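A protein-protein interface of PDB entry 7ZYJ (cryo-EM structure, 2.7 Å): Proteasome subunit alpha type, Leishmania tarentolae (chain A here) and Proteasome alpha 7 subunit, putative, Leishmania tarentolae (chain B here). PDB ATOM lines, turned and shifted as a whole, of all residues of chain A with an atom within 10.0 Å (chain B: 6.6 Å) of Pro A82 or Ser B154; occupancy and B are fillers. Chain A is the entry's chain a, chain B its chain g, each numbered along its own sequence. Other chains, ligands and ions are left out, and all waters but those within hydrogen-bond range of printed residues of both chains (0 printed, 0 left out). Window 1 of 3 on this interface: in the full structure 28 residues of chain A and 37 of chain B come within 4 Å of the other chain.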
ATOM      1  N   ALA A  28       9.586 -20.623 -31.402  1.00  0.00           N
ATOM      2  CA  ALA A  28       8.603 -20.867 -30.356  1.00  0.00           C
ATOM      3  C   ALA A  28       8.260 -22.344 -30.233  1.00  0.00           C
ATOM      4  O   ALA A  28       7.729 -22.761 -29.199  1.00  0.00           O
ATOM      5  CB  ALA A  28       7.334 -20.055 -30.621  1.00  0.00           C
ATOM      6  N   TYR A  31      11.083 -23.568 -27.949  1.00  0.00           N
ATOM      7  CA  TYR A  31      11.186 -22.783 -26.722  1.00  0.00           C
ATOM      8  C   TYR A  31      10.748 -23.546 -25.471  1.00  0.00           C
ATOM      9  O   TYR A  31      11.458 -23.494 -24.459  1.00  0.00           O
ATOM     10  CB  TYR A  31      10.381 -21.487 -26.845  1.00  0.00           C
ATOM     11  CG  TYR A  31      10.540 -20.580 -25.647  1.00  0.00           C
ATOM     12  CD1 TYR A  31      11.719 -19.878 -25.437  1.00  0.00           C
ATOM     13  CD2 TYR A  31       9.518 -20.439 -24.719  1.00  0.00           C
ATOM     14  CE1 TYR A  31      11.871 -19.054 -24.339  1.00  0.00           C
ATOM     15  CE2 TYR A  31       9.662 -19.617 -23.619  1.00  0.00           C
ATOM     16  CZ  TYR A  31      10.840 -18.929 -23.433  1.00  0.00           C
ATOM     17  OH  TYR A  31      10.988 -18.109 -22.338  1.00  0.00           O
ATOM     18  N   PRO A  32       9.606 -24.251 -25.470  1.00  0.00           N
ATOM     19  CA  PRO A  32       9.185 -24.942 -24.238  1.00  0.00           C
ATOM     20  C   PRO A  32      10.132 -26.042 -23.788  1.00  0.00           C
ATOM     21  O   PRO A  32      10.057 -26.452 -22.622  1.00  0.00           O
ATOM     22  CB  PRO A  32       7.809 -25.517 -24.605  1.00  0.00           C
ATOM     23  CG  PRO A  32       7.360 -24.726 -25.775  1.00  0.00           C
ATOM     24  CD  PRO A  32       8.602 -24.421 -26.535  1.00  0.00           C
ATOM     25  N   VAL A  63      -3.067 -32.205 -18.264  1.00  0.00           N
ATOM     26  CA  VAL A  63      -2.326 -31.603 -19.365  1.00  0.00           C
ATOM     27  C   VAL A  63      -1.794 -32.702 -20.277  1.00  0.00           C
ATOM     28  O   VAL A  63      -1.209 -33.689 -19.814  1.00  0.00           O
ATOM     29  CB  VAL A  63      -1.196 -30.702 -18.838  1.00  0.00           C
ATOM     30  CG1 VAL A  63      -1.777 -29.552 -18.040  1.00  0.00           C
ATOM     31  CG2 VAL A  63      -0.226 -31.492 -17.973  1.00  0.00           C
ATOM     32  N   THR A  64      -2.027 -32.549 -21.578  1.00  0.00           N
ATOM     33  CA  THR A  64      -1.538 -33.503 -22.560  1.00  0.00           C
ATOM     34  C   THR A  64      -1.302 -32.779 -23.876  1.00  0.00           C
ATOM     35  O   THR A  64      -1.936 -31.764 -24.171  1.00  0.00           O
ATOM     36  CB  THR A  64      -2.517 -34.669 -22.757  1.00  0.00           C
ATOM     37  OG1 THR A  64      -1.976 -35.597 -23.704  1.00  0.00           O
ATOM     38  CG2 THR A  64      -3.860 -34.162 -23.260  1.00  0.00           C
ATOM     39  N   ALA A  65      -0.369 -33.312 -24.662  1.00  0.00           N
ATOM     40  CA  ALA A  65      -0.102 -32.804 -25.997  1.00  0.00           C
ATOM     41  C   ALA A  65      -0.703 -33.666 -27.094  1.00  0.00           C
ATOM     42  O   ALA A  65      -0.578 -33.316 -28.272  1.00  0.00           O
ATOM     43  CB  ALA A  65       1.410 -32.669 -26.227  1.00  0.00           C
ATOM     44  N   TYR A  67      -3.981 -35.114 -28.984  1.00  0.00           N
ATOM     45  CA  TYR A  67      -5.377 -34.770 -29.190  1.00  0.00           C
ATOM     46  C   TYR A  67      -5.990 -35.687 -30.237  1.00  0.00           C
ATOM     47  O   TYR A  67      -5.305 -36.177 -31.139  1.00  0.00           O
ATOM     48  CB  TYR A  67      -5.541 -33.313 -29.637  1.00  0.00           C
ATOM     49  CG  TYR A  67      -4.889 -32.301 -28.727  1.00  0.00           C
ATOM     50  CD1 TYR A  67      -3.568 -31.916 -28.915  1.00  0.00           C
ATOM     51  CD2 TYR A  67      -5.599 -31.719 -27.687  1.00  0.00           C
ATOM     52  CE1 TYR A  67      -2.972 -30.987 -28.087  1.00  0.00           C
ATOM     53  CE2 TYR A  67      -5.012 -30.788 -26.855  1.00  0.00           C
ATOM     54  CZ  TYR A  67      -3.699 -30.426 -27.059  1.00  0.00           C
ATOM     55  OH  TYR A  67      -3.111 -29.499 -26.231  1.00  0.00           O
ATOM     56  N   MET A  77       0.860 -31.780 -30.755  1.00  0.00           N
ATOM     57  CA  MET A  77       1.268 -30.389 -30.912  1.00  0.00           C
ATOM     58  C   MET A  77       2.562 -30.161 -30.143  1.00  0.00           C
ATOM     59  O   MET A  77       2.658 -30.518 -28.964  1.00  0.00           O
ATOM     60  CB  MET A  77       0.174 -29.442 -30.422  1.00  0.00           C
ATOM     61  CG  MET A  77      -1.060 -29.409 -31.305  1.00  0.00           C
ATOM     62  SD  MET A  77      -0.799 -28.455 -32.812  1.00  0.00           S
ATOM     63  CE  MET A  77      -2.243 -28.918 -33.763  1.00  0.00           C
ATOM     64  N   THR A  78       3.548 -29.569 -30.809  1.00  0.00           N
ATOM     65  CA  THR A  78       4.841 -29.268 -30.210  1.00  0.00           C
ATOM     66  C   THR A  78       5.091 -27.770 -30.313  1.00  0.00           C
ATOM     67  O   THR A  78       5.167 -27.226 -31.419  1.00  0.00           O
ATOM     68  CB  THR A  78       5.962 -30.042 -30.903  1.00  0.00           C
ATOM     69  OG1 THR A  78       5.626 -31.433 -30.945  1.00  0.00           O
ATOM     70  CG2 THR A  78       7.268 -29.868 -30.149  1.00  0.00           C
ATOM     71  N   GLY A  79       5.232 -27.112 -29.166  1.00  0.00           N
ATOM     72  CA  GLY A  79       5.449 -25.680 -29.145  1.00  0.00           C
ATOM     73  C   GLY A  79       4.610 -24.965 -28.108  1.00  0.00           C
ATOM     74  O   GLY A  79       4.360 -25.504 -27.027  1.00  0.00           O
ATOM     75  N   ARG A  80       4.183 -23.743 -28.424  1.00  0.00           N
ATOM     76  CA  ARG A  80       3.340 -22.975 -27.516  1.00  0.00           C
ATOM     77  C   ARG A  80       2.052 -23.737 -27.231  1.00  0.00           C
ATOM     78  O   ARG A  80       1.230 -23.938 -28.129  1.00  0.00           O
ATOM     79  CB  ARG A  80       3.036 -21.607 -28.125  1.00  0.00           C
ATOM     80  CG  ARG A  80       2.635 -20.542 -27.121  1.00  0.00           C
ATOM     81  CD  ARG A  80       2.621 -19.164 -27.763  1.00  0.00           C
ATOM     82  NE  ARG A  80       1.919 -18.182 -26.943  1.00  0.00           N
ATOM     83  CZ  ARG A  80       2.494 -17.436 -26.010  1.00  0.00           C
ATOM     84  NH1 ARG A  80       3.789 -17.523 -25.757  1.00  0.00           N
ATOM     85  NH2 ARG A  80       1.752 -16.580 -25.316  1.00  0.00           N
ATOM     86  N   ALA A  81       1.880 -24.155 -25.976  1.00  0.00           N
ATOM     87  CA  ALA A  81       0.792 -25.071 -25.638  1.00  0.00           C
ATOM     88  C   ALA A  81      -0.588 -24.529 -25.989  1.00  0.00           C
ATOM     89  O   ALA A  81      -1.369 -25.268 -26.613  1.00  0.00           O
ATOM     90  CB  ALA A  81       0.885 -25.454 -24.157  1.00  0.00           C
ATOM     91  N   PRO A  82      -0.969 -23.295 -25.629  1.00  0.00           N
ATOM     92  CA  PRO A  82      -2.299 -22.819 -26.047  1.00  0.00           C
ATOM     93  C   PRO A  82      -2.458 -22.737 -27.556  1.00  0.00           C
ATOM     94  O   PRO A  82      -3.502 -23.141 -28.085  1.00  0.00           O
ATOM     95  CB  PRO A  82      -2.402 -21.438 -25.386  1.00  0.00           C
ATOM     96  CG  PRO A  82      -1.001 -21.038 -25.107  1.00  0.00           C
ATOM     97  CD  PRO A  82      -0.281 -22.299 -24.787  1.00  0.00           C
ATOM     98  N   ASP A  83      -1.431 -22.256 -28.262  1.00  0.00           N
ATOM     99  CA  ASP A  83      -1.516 -22.077 -29.708  1.00  0.00           C
ATOM    100  C   ASP A  83      -1.915 -23.372 -30.397  1.00  0.00           C
ATOM    101  O   ASP A  83      -2.884 -23.416 -31.163  1.00  0.00           O
ATOM    102  CB  ASP A  83      -0.177 -21.576 -30.251  1.00  0.00           C
ATOM    103  CG  ASP A  83      -0.029 -20.078 -30.145  1.00  0.00           C
ATOM    104  OD1 ASP A  83      -0.836 -19.445 -29.434  1.00  0.00           O
ATOM    105  OD2 ASP A  83       0.897 -19.526 -30.774  1.00  0.00           O
ATOM    106  N   GLY A  84      -1.187 -24.452 -30.103  1.00  0.00           N
ATOM    107  CA  GLY A  84      -1.528 -25.740 -30.680  1.00  0.00           C
ATOM    108  C   GLY A  84      -2.958 -26.133 -30.382  1.00  0.00           C
ATOM    109  O   GLY A  84      -3.680 -26.609 -31.262  1.00  0.00           O
ATOM    110  N   ARG A  85      -3.397 -25.900 -29.141  1.00  0.00           N
ATOM    111  CA  ARG A  85      -4.787 -26.158 -28.787  1.00  0.00           C
ATOM    112  C   ARG A  85      -5.722 -25.475 -29.772  1.00  0.00           C
ATOM    113  O   ARG A  85      -6.606 -26.115 -30.355  1.00  0.00           O
ATOM    114  CB  ARG A  85      -5.059 -25.681 -27.360  1.00  0.00           C
ATOM    115  CG  ARG A  85      -6.496 -25.854 -26.907  1.00  0.00           C
ATOM    116  CD  ARG A  85      -6.798 -27.291 -26.525  1.00  0.00           C
ATOM    117  NE  ARG A  85      -8.227 -27.575 -26.592  1.00  0.00           N
ATOM    118  CZ  ARG A  85      -8.808 -28.628 -26.034  1.00  0.00           C
ATOM    119  NH1 ARG A  85      -8.112 -29.521 -25.351  1.00  0.00           N
ATOM    120  NH2 ARG A  85     -10.122 -28.788 -26.164  1.00  0.00           N
ATOM    121  N   ALA A  86      -5.491 -24.183 -30.022  1.00  0.00           N
ATOM    122  CA  ALA A  86      -6.306 -23.456 -30.986  1.00  0.00           C
ATOM    123  C   ALA A  86      -6.301 -24.164 -32.331  1.00  0.00           C
ATOM    124  O   ALA A  86      -7.363 -24.437 -32.906  1.00  0.00           O
ATOM    125  CB  ALA A  86      -5.800 -22.021 -31.126  1.00  0.00           C
ATOM    126  N   LEU A  87      -5.112 -24.534 -32.814  1.00  0.00           N
ATOM    127  CA  LEU A  87      -5.030 -25.223 -34.095  1.00  0.00           C
ATOM    128  C   LEU A  87      -5.826 -26.514 -34.057  1.00  0.00           C
ATOM    129  O   LEU A  87      -6.586 -26.816 -34.987  1.00  0.00           O
ATOM    130  CB  LEU A  87      -3.572 -25.497 -34.466  1.00  0.00           C
ATOM    131  CG  LEU A  87      -2.782 -24.306 -35.001  1.00  0.00           C
ATOM    132  CD1 LEU A  87      -1.464 -24.769 -35.586  1.00  0.00           C
ATOM    133  CD2 LEU A  87      -3.598 -23.560 -36.044  1.00  0.00           C
ATOM    134  N   VAL A  88      -5.712 -27.261 -32.954  1.00  0.00           N
ATOM    135  CA  VAL A  88      -6.482 -28.494 -32.825  1.00  0.00           C
ATOM    136  C   VAL A  88      -7.953 -28.188 -33.032  1.00  0.00           C
ATOM    137  O   VAL A  88      -8.628 -28.815 -33.862  1.00  0.00           O
ATOM    138  CB  VAL A  88      -6.229 -29.153 -31.458  1.00  0.00           C
ATOM    139  CG1 VAL A  88      -7.293 -30.200 -31.171  1.00  0.00           C
ATOM    140  CG2 VAL A  88      -4.849 -29.776 -31.417  1.00  0.00           C
ATOM    141  N   GLN A  89      -8.442 -27.148 -32.352  1.00  0.00           N
ATOM    142  CA  GLN A  89      -9.836 -26.757 -32.504  1.00  0.00           C
ATOM    143  C   GLN A  89     -10.174 -26.576 -33.972  1.00  0.00           C
ATOM    144  O   GLN A  89     -11.093 -27.222 -34.486  1.00  0.00           O
ATOM    145  CB  GLN A  89     -10.119 -25.479 -31.715  1.00  0.00           C
ATOM    146  CG  GLN A  89     -10.001 -25.659 -30.217  1.00  0.00           C
ATOM    147  CD  GLN A  89     -10.741 -26.887 -29.727  1.00  0.00           C
ATOM    148  OE1 GLN A  89     -11.968 -26.949 -29.779  1.00  0.00           O
ATOM    149  NE2 GLN A  89      -9.993 -27.875 -29.251  1.00  0.00           N
ATOM    150  N   ARG A  90      -9.367 -25.784 -34.687  1.00  0.00           N
ATOM    151  CA  ARG A  90      -9.653 -25.521 -36.094  1.00  0.00           C
ATOM    152  C   ARG A  90      -9.761 -26.821 -36.873  1.00  0.00           C
ATOM    153  O   ARG A  90     -10.732 -27.036 -37.612  1.00  0.00           O
ATOM    154  CB  ARG A  90      -8.577 -24.618 -36.700  1.00  0.00           C
ATOM    155  CG  ARG A  90      -8.149 -23.446 -35.831  1.00  0.00           C
ATOM    156  CD  ARG A  90      -9.038 -22.226 -36.039  1.00  0.00           C
ATOM    157  NE  ARG A  90     -10.401 -22.441 -35.572  1.00  0.00           N
ATOM    158  CZ  ARG A  90     -10.780 -22.370 -34.303  1.00  0.00           C
ATOM    159  NH1 ARG A  90      -9.920 -22.075 -33.340  1.00  0.00           N
ATOM    160  NH2 ARG A  90     -12.052 -22.600 -33.991  1.00  0.00           N
ATOM    161  N   ARG A 129      -0.957 -13.293 -36.028  1.00  0.00           N
ATOM    162  CA  ARG A 129       0.269 -13.911 -35.541  1.00  0.00           C
ATOM    163  C   ARG A 129       0.279 -15.391 -35.883  1.00  0.00           C
ATOM    164  O   ARG A 129      -0.725 -16.078 -35.650  1.00  0.00           O
ATOM    165  CB  ARG A 129       0.400 -13.735 -34.031  1.00  0.00           C
ATOM    166  CG  ARG A 129       1.761 -14.121 -33.483  1.00  0.00           C
ATOM    167  CD  ARG A 129       1.759 -14.147 -31.968  1.00  0.00           C
ATOM    168  NE  ARG A 129       1.659 -15.504 -31.447  1.00  0.00           N
ATOM    169  CZ  ARG A 129       0.801 -15.886 -30.511  1.00  0.00           C
ATOM    170  NH1 ARG A 129      -0.054 -15.036 -29.968  1.00  0.00           N
ATOM    171  NH2 ARG A 129       0.803 -17.152 -30.110  1.00  0.00           N
ATOM    172  N   PRO A 130       1.372 -15.914 -36.434  1.00  0.00           N
ATOM    173  CA  PRO A 130       1.438 -17.352 -36.705  1.00  0.00           C
ATOM    174  C   PRO A 130       1.410 -18.161 -35.419  1.00  0.00           C
ATOM    175  O   PRO A 130       1.831 -17.700 -34.356  1.00  0.00           O
ATOM    176  CB  PRO A 130       2.778 -17.518 -37.435  1.00  0.00           C
ATOM    177  CG  PRO A 130       3.139 -16.146 -37.908  1.00  0.00           C
ATOM    178  CD  PRO A 130       2.577 -15.208 -36.894  1.00  0.00           C
ATOM    179  N   MET A 131       0.898 -19.382 -35.526  1.00  0.00           N
ATOM    180  CA  MET A 131       0.858 -20.305 -34.399  1.00  0.00           C
ATOM    181  C   MET A 131       2.228 -20.953 -34.248  1.00  0.00           C
ATOM    182  O   MET A 131       2.677 -21.683 -35.138  1.00  0.00           O
ATOM    183  CB  MET A 131      -0.224 -21.364 -34.603  1.00  0.00           C
ATOM    184  CG  MET A 131      -1.644 -20.817 -34.655  1.00  0.00           C
ATOM    185  SD  MET A 131      -2.298 -20.330 -33.046  1.00  0.00           S
ATOM    186  CE  MET A 131      -1.951 -18.574 -33.041  1.00  0.00           C
ATOM    187  N   GLY A 132       2.888 -20.687 -33.125  1.00  0.00           N
ATOM    188  CA  GLY A 132       4.231 -21.186 -32.909  1.00  0.00           C
ATOM    189  C   GLY A 132       4.280 -22.639 -32.489  1.00  0.00           C
ATOM    190  O   GLY A 132       4.872 -22.975 -31.460  1.00  0.00           O
ATOM    191  N   VAL A 133       3.658 -23.514 -33.278  1.00  0.00           N
ATOM    192  CA  VAL A 133       3.655 -24.946 -33.010  1.00  0.00           C
ATOM    193  C   VAL A 133       3.864 -25.700 -34.315  1.00  0.00           C
ATOM    194  O   VAL A 133       3.573 -25.195 -35.403  1.00  0.00           O
ATOM    195  CB  VAL A 133       2.350 -25.417 -32.330  1.00  0.00           C
ATOM    196  CG1 VAL A 133       2.213 -24.809 -30.955  1.00  0.00           C
ATOM    197  CG2 VAL A 133       1.155 -25.058 -33.183  1.00  0.00           C
ATOM    198  N   VAL B  24       2.045 -10.876 -23.539  1.00  0.00           N
ATOM    199  CA  VAL B  24       1.474 -11.899 -22.672  1.00  0.00           C
ATOM    200  C   VAL B  24       2.279 -12.017 -21.384  1.00  0.00           C
ATOM    201  O   VAL B  24       1.715 -12.182 -20.296  1.00  0.00           O
ATOM    202  CB  VAL B  24       1.397 -13.242 -23.416  1.00  0.00           C
ATOM    203  CG1 VAL B  24       0.781 -14.292 -22.527  1.00  0.00           C
ATOM    204  CG2 VAL B  24       0.598 -13.090 -24.698  1.00  0.00           C
ATOM    205  N   GLY B 117      -9.813 -21.248 -21.610  1.00  0.00           N
ATOM    206  CA  GLY B 117      -8.483 -21.104 -22.175  1.00  0.00           C
ATOM    207  C   GLY B 117      -8.504 -20.672 -23.627  1.00  0.00           C
ATOM    208  O   GLY B 117      -7.692 -19.845 -24.049  1.00  0.00           O
ATOM    209  N   MET B 120      -9.390 -16.966 -23.689  1.00  0.00           N
ATOM    210  CA  MET B 120      -8.282 -16.115 -23.267  1.00  0.00           C
ATOM    211  C   MET B 120      -7.150 -16.112 -24.287  1.00  0.00           C
ATOM    212  O   MET B 120      -6.448 -15.105 -24.428  1.00  0.00           O
ATOM    213  CB  MET B 120      -7.767 -16.565 -21.900  1.00  0.00           C
ATOM    214  CG  MET B 120      -8.760 -16.359 -20.771  1.00  0.00           C
ATOM    215  SD  MET B 120      -8.157 -16.975 -19.190  1.00  0.00           S
ATOM    216  CE  MET B 120      -6.874 -15.781 -18.831  1.00  0.00           C
ATOM    217  N   HIS B 121      -6.957 -17.223 -25.001  1.00  0.00           N
ATOM    218  CA  HIS B 121      -5.875 -17.304 -25.975  1.00  0.00           C
ATOM    219  C   HIS B 121      -6.151 -16.452 -27.207  1.00  0.00           C
ATOM    220  O   HIS B 121      -5.213 -15.931 -27.818  1.00  0.00           O
ATOM    221  CB  HIS B 121      -5.648 -18.763 -26.377  1.00  0.00           C
ATOM    222  CG  HIS B 121      -4.739 -18.930 -27.553  1.00  0.00           C
ATOM    223  ND1 HIS B 121      -5.208 -19.128 -28.834  1.00  0.00           N
ATOM    224  CD2 HIS B 121      -3.389 -18.929 -27.643  1.00  0.00           C
ATOM    225  CE1 HIS B 121      -4.185 -19.243 -29.661  1.00  0.00           C
ATOM    226  NE2 HIS B 121      -3.070 -19.124 -28.964  1.00  0.00           N
ATOM    227  N   ALA B 122      -7.423 -16.301 -27.586  1.00  0.00           N
ATOM    228  CA  ALA B 122      -7.761 -15.557 -28.793  1.00  0.00           C
ATOM    229  C   ALA B 122      -7.359 -14.090 -28.707  1.00  0.00           C
ATOM    230  O   ALA B 122      -7.191 -13.444 -29.746  1.00  0.00           O
ATOM    231  CB  ALA B 122      -9.258 -15.670 -29.078  1.00  0.00           C
ATOM    232  N   THR B 124      -4.521 -13.079 -27.492  1.00  0.00           N
ATOM    233  CA  THR B 124      -3.069 -13.018 -27.572  1.00  0.00           C
ATOM    234  C   THR B 124      -2.558 -13.203 -28.994  1.00  0.00           C
ATOM    235  O   THR B 124      -1.347 -13.331 -29.196  1.00  0.00           O
ATOM    236  CB  THR B 124      -2.444 -14.072 -26.656  1.00  0.00           C
ATOM    237  OG1 THR B 124      -2.735 -15.380 -27.164  1.00  0.00           O
ATOM    238  CG2 THR B 124      -3.002 -13.953 -25.250  1.00  0.00           C
ATOM    239  N   PRO B 131      -3.917  -9.067 -24.133  1.00  0.00           N
ATOM    240  CA  PRO B 131      -4.264 -10.228 -23.310  1.00  0.00           C
ATOM    241  C   PRO B 131      -4.899  -9.803 -21.998  1.00  0.00           C
ATOM    242  O   PRO B 131      -4.693  -8.694 -21.500  1.00  0.00           O
ATOM    243  CB  PRO B 131      -2.917 -10.923 -23.071  1.00  0.00           C
ATOM    244  CG  PRO B 131      -1.943 -10.250 -23.987  1.00  0.00           C
ATOM    245  CD  PRO B 131      -2.461  -8.871 -24.199  1.00  0.00           C
ATOM    246  N   PHE B 132      -5.692 -10.712 -21.441  1.00  0.00           N
ATOM    247  CA  PHE B 132      -6.310 -10.465 -20.149  1.00  0.00           C
ATOM    248  C   PHE B 132      -5.248 -10.404 -19.061  1.00  0.00           C
ATOM    249  O   PHE B 132      -4.288 -11.179 -19.062  1.00  0.00           O
ATOM    250  CB  PHE B 132      -7.331 -11.556 -19.830  1.00  0.00           C
ATOM    251  CG  PHE B 132      -8.528 -11.544 -20.733  1.00  0.00           C
ATOM    252  CD1 PHE B 132      -9.599 -10.707 -20.473  1.00  0.00           C
ATOM    253  CD2 PHE B 132      -8.583 -12.370 -21.842  1.00  0.00           C
ATOM    254  CE1 PHE B 132     -10.702 -10.695 -21.302  1.00  0.00           C
ATOM    255  CE2 PHE B 132      -9.681 -12.361 -22.674  1.00  0.00           C
ATOM    256  CZ  PHE B 132     -10.742 -11.522 -22.404  1.00  0.00           C
ATOM    257  N   SER B 151      -6.324 -21.186 -15.679  1.00  0.00           N
ATOM    258  CA  SER B 151      -6.149 -20.610 -17.002  1.00  0.00           C
ATOM    259  C   SER B 151      -5.291 -19.359 -16.884  1.00  0.00           C
ATOM    260  O   SER B 151      -5.672 -18.398 -16.204  1.00  0.00           O
ATOM    261  CB  SER B 151      -7.498 -20.274 -17.642  1.00  0.00           C
ATOM    262  OG  SER B 151      -7.326 -19.743 -18.944  1.00  0.00           O
ATOM    263  N   ASP B 152      -4.138 -19.396 -17.537  1.00  0.00           N
ATOM    264  CA  ASP B 152      -3.074 -18.420 -17.690  1.00  0.00           C
ATOM    265  C   ASP B 152      -3.487 -17.367 -18.709  1.00  0.00           C
ATOM    266  O   ASP B 152      -4.168 -17.678 -19.690  1.00  0.00           O
ATOM    267  CB  ASP B 152      -1.803 -19.153 -18.153  1.00  0.00           C
ATOM    268  CG  ASP B 152      -0.548 -18.288 -18.152  1.00  0.00           C
ATOM    269  OD1 ASP B 152      -0.599 -17.091 -17.825  1.00  0.00           O
ATOM    270  OD2 ASP B 152       0.523 -18.834 -18.490  1.00  0.00           O
ATOM    271  N   PRO B 153      -3.127 -16.097 -18.495  1.00  0.00           N
ATOM    272  CA  PRO B 153      -3.304 -15.095 -19.560  1.00  0.00           C
ATOM    273  C   PRO B 153      -2.796 -15.529 -20.926  1.00  0.00           C
ATOM    274  O   PRO B 153      -3.290 -15.028 -21.944  1.00  0.00           O
ATOM    275  CB  PRO B 153      -2.520 -13.900 -19.014  1.00  0.00           C
ATOM    276  CG  PRO B 153      -2.775 -13.975 -17.547  1.00  0.00           C
ATOM    277  CD  PRO B 153      -2.913 -15.446 -17.189  1.00  0.00           C
ATOM    278  N   SER B 154      -1.826 -16.442 -20.987  1.00  0.00           N
ATOM    279  CA  SER B 154      -1.424 -17.020 -22.261  1.00  0.00           C
ATOM    280  C   SER B 154      -2.479 -17.948 -22.844  1.00  0.00           C
ATOM    281  O   SER B 154      -2.368 -18.326 -24.015  1.00  0.00           O
ATOM    282  CB  SER B 154      -0.105 -17.776 -22.103  1.00  0.00           C
ATOM    283  OG  SER B 154      -0.255 -18.873 -21.224  1.00  0.00           O
ATOM    284  N   GLY B 155      -3.495 -18.313 -22.069  1.00  0.00           N
ATOM    285  CA  GLY B 155      -4.539 -19.199 -22.533  1.00  0.00           C
ATOM    286  C   GLY B 155      -4.300 -20.670 -22.294  1.00  0.00           C
ATOM    287  O   GLY B 155      -5.138 -21.486 -22.695  1.00  0.00           O
ATOM    288  N   THR B 156      -3.193 -21.043 -21.656  1.00  0.00           N
ATOM    289  CA  THR B 156      -2.946 -22.442 -21.344  1.00  0.00           C
ATOM    290  C   THR B 156      -3.636 -22.812 -20.036  1.00  0.00           C
ATOM    291  O   THR B 156      -3.615 -22.044 -19.069  1.00  0.00           O
ATOM    292  CB  THR B 156      -1.445 -22.732 -21.265  1.00  0.00           C
ATOM    293  OG1 THR B 156      -1.238 -24.110 -20.933  1.00  0.00           O
ATOM    294  CG2 THR B 156      -0.766 -21.860 -20.227  1.00  0.00           C
ATOM    295  N   VAL B 157      -4.272 -23.978 -20.020  1.00  0.00           N
ATOM    296  CA  VAL B 157      -5.018 -24.455 -18.865  1.00  0.00           C
ATOM    297  C   VAL B 157      -4.310 -25.673 -18.296  1.00  0.00           C
ATOM    298  O   VAL B 157      -3.797 -26.520 -19.036  1.00  0.00           O
ATOM    299  CB  VAL B 157      -6.478 -24.794 -19.231  1.00  0.00           C
ATOM    300  CG1 VAL B 157      -7.306 -24.983 -17.975  1.00  0.00           C
ATOM    301  CG2 VAL B 157      -7.066 -23.707 -20.108  1.00  0.00           C
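Hydrophobic or aromatic side chains of chain A within 4 Å of the printed part of chain B: Val A63, Pro A82 and Ala A86.
Printed residues of chain B that touch a printed residue of chain A: Val B24, His B121, Thr B124, Ser B154, Gly B155, Thr B156 and Val B157.
Hydrophobic or aromatic side chains of chain B within 4 Å of the printed part of chain A: Val B24 and His B121.
Among the printed residues, 10 pairs touch across the chains.
NE2 of His B121 lies close to OD1 of Asp A83 (2.3 Å).
The backbone carbonyl oxygen of Thr B124 lies close to the guanidinium group of Arg A129 (2.3 Å).
NE of Arg A80 is in salt-bridge range of OD1 of Asp A83, 3.9 Å away.
N of Arg A80 sits at hydrogen-bond distance from O of Gly A132 (3.2 Å).
The side-chain carboxylate (OD2) of Asp A83 is in salt-bridge range of the guanidinium group (NH2) of Arg A129 (2.5 Å).
OD2 of Asp A83 sits at hydrogen-bond distance from N of Gly A132 (3.3 Å).
O of His B121 lies within hydrogen-bond range of OG1 of Thr B124 (2.6 Å).
The side-chain carboxylate (OD2) of Asp B152 is in hydrogen-bond range of the side-chain hydroxyl (OG) of Ser B154 (2.8 Å).
Among the printed residues, pairs that only touch across the chains: Pro A82 with Ser B154, Pro A82 with His B121, Ala A86 with His B121, Pro A82 with Gly B155, Arg A80 with Val B24, Pro A82 with Thr B156, Val A63 with Val B157 and Arg A80 with Ser B154.
Of chain B, only His B121, Ser B154, Gly B155 and Thr B156 come within 4 Å of Pro A82.
Of the printed residues of chain B, Ala A86 touches His B121 (3.5 Å).
Leu A87 touches none of the printed residues of chain B.
Of the printed residues of chain B, Arg A129 touches Thr B124 (2.3 Å).
Gly A132 touches none of the printed residues of chain B.
Of chain A, only Pro A82 (3.5 Å), Asp A83 (2.3 Å) and Ala A86 (3.5 Å) come within 4 Å of His B121.
No residue of chain A comes within 4 Å of Asp B152.
No residue of chain A comes within 4 Å of Pro B153.
Printed residues of chain A within 4 Å of Gly B155: Pro A82.
Thr B156 touches one residue of chain A.
Of the printed residues of chain A, Val B157 touches Val A63 (3.8 Å).
The nearest residue of chain B that does not touch Pro A82 is Gly B117 (5.7 Å).
The nearest printed residue of chain A that does not touch Val B24 is Arg A129 (5.7 Å).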
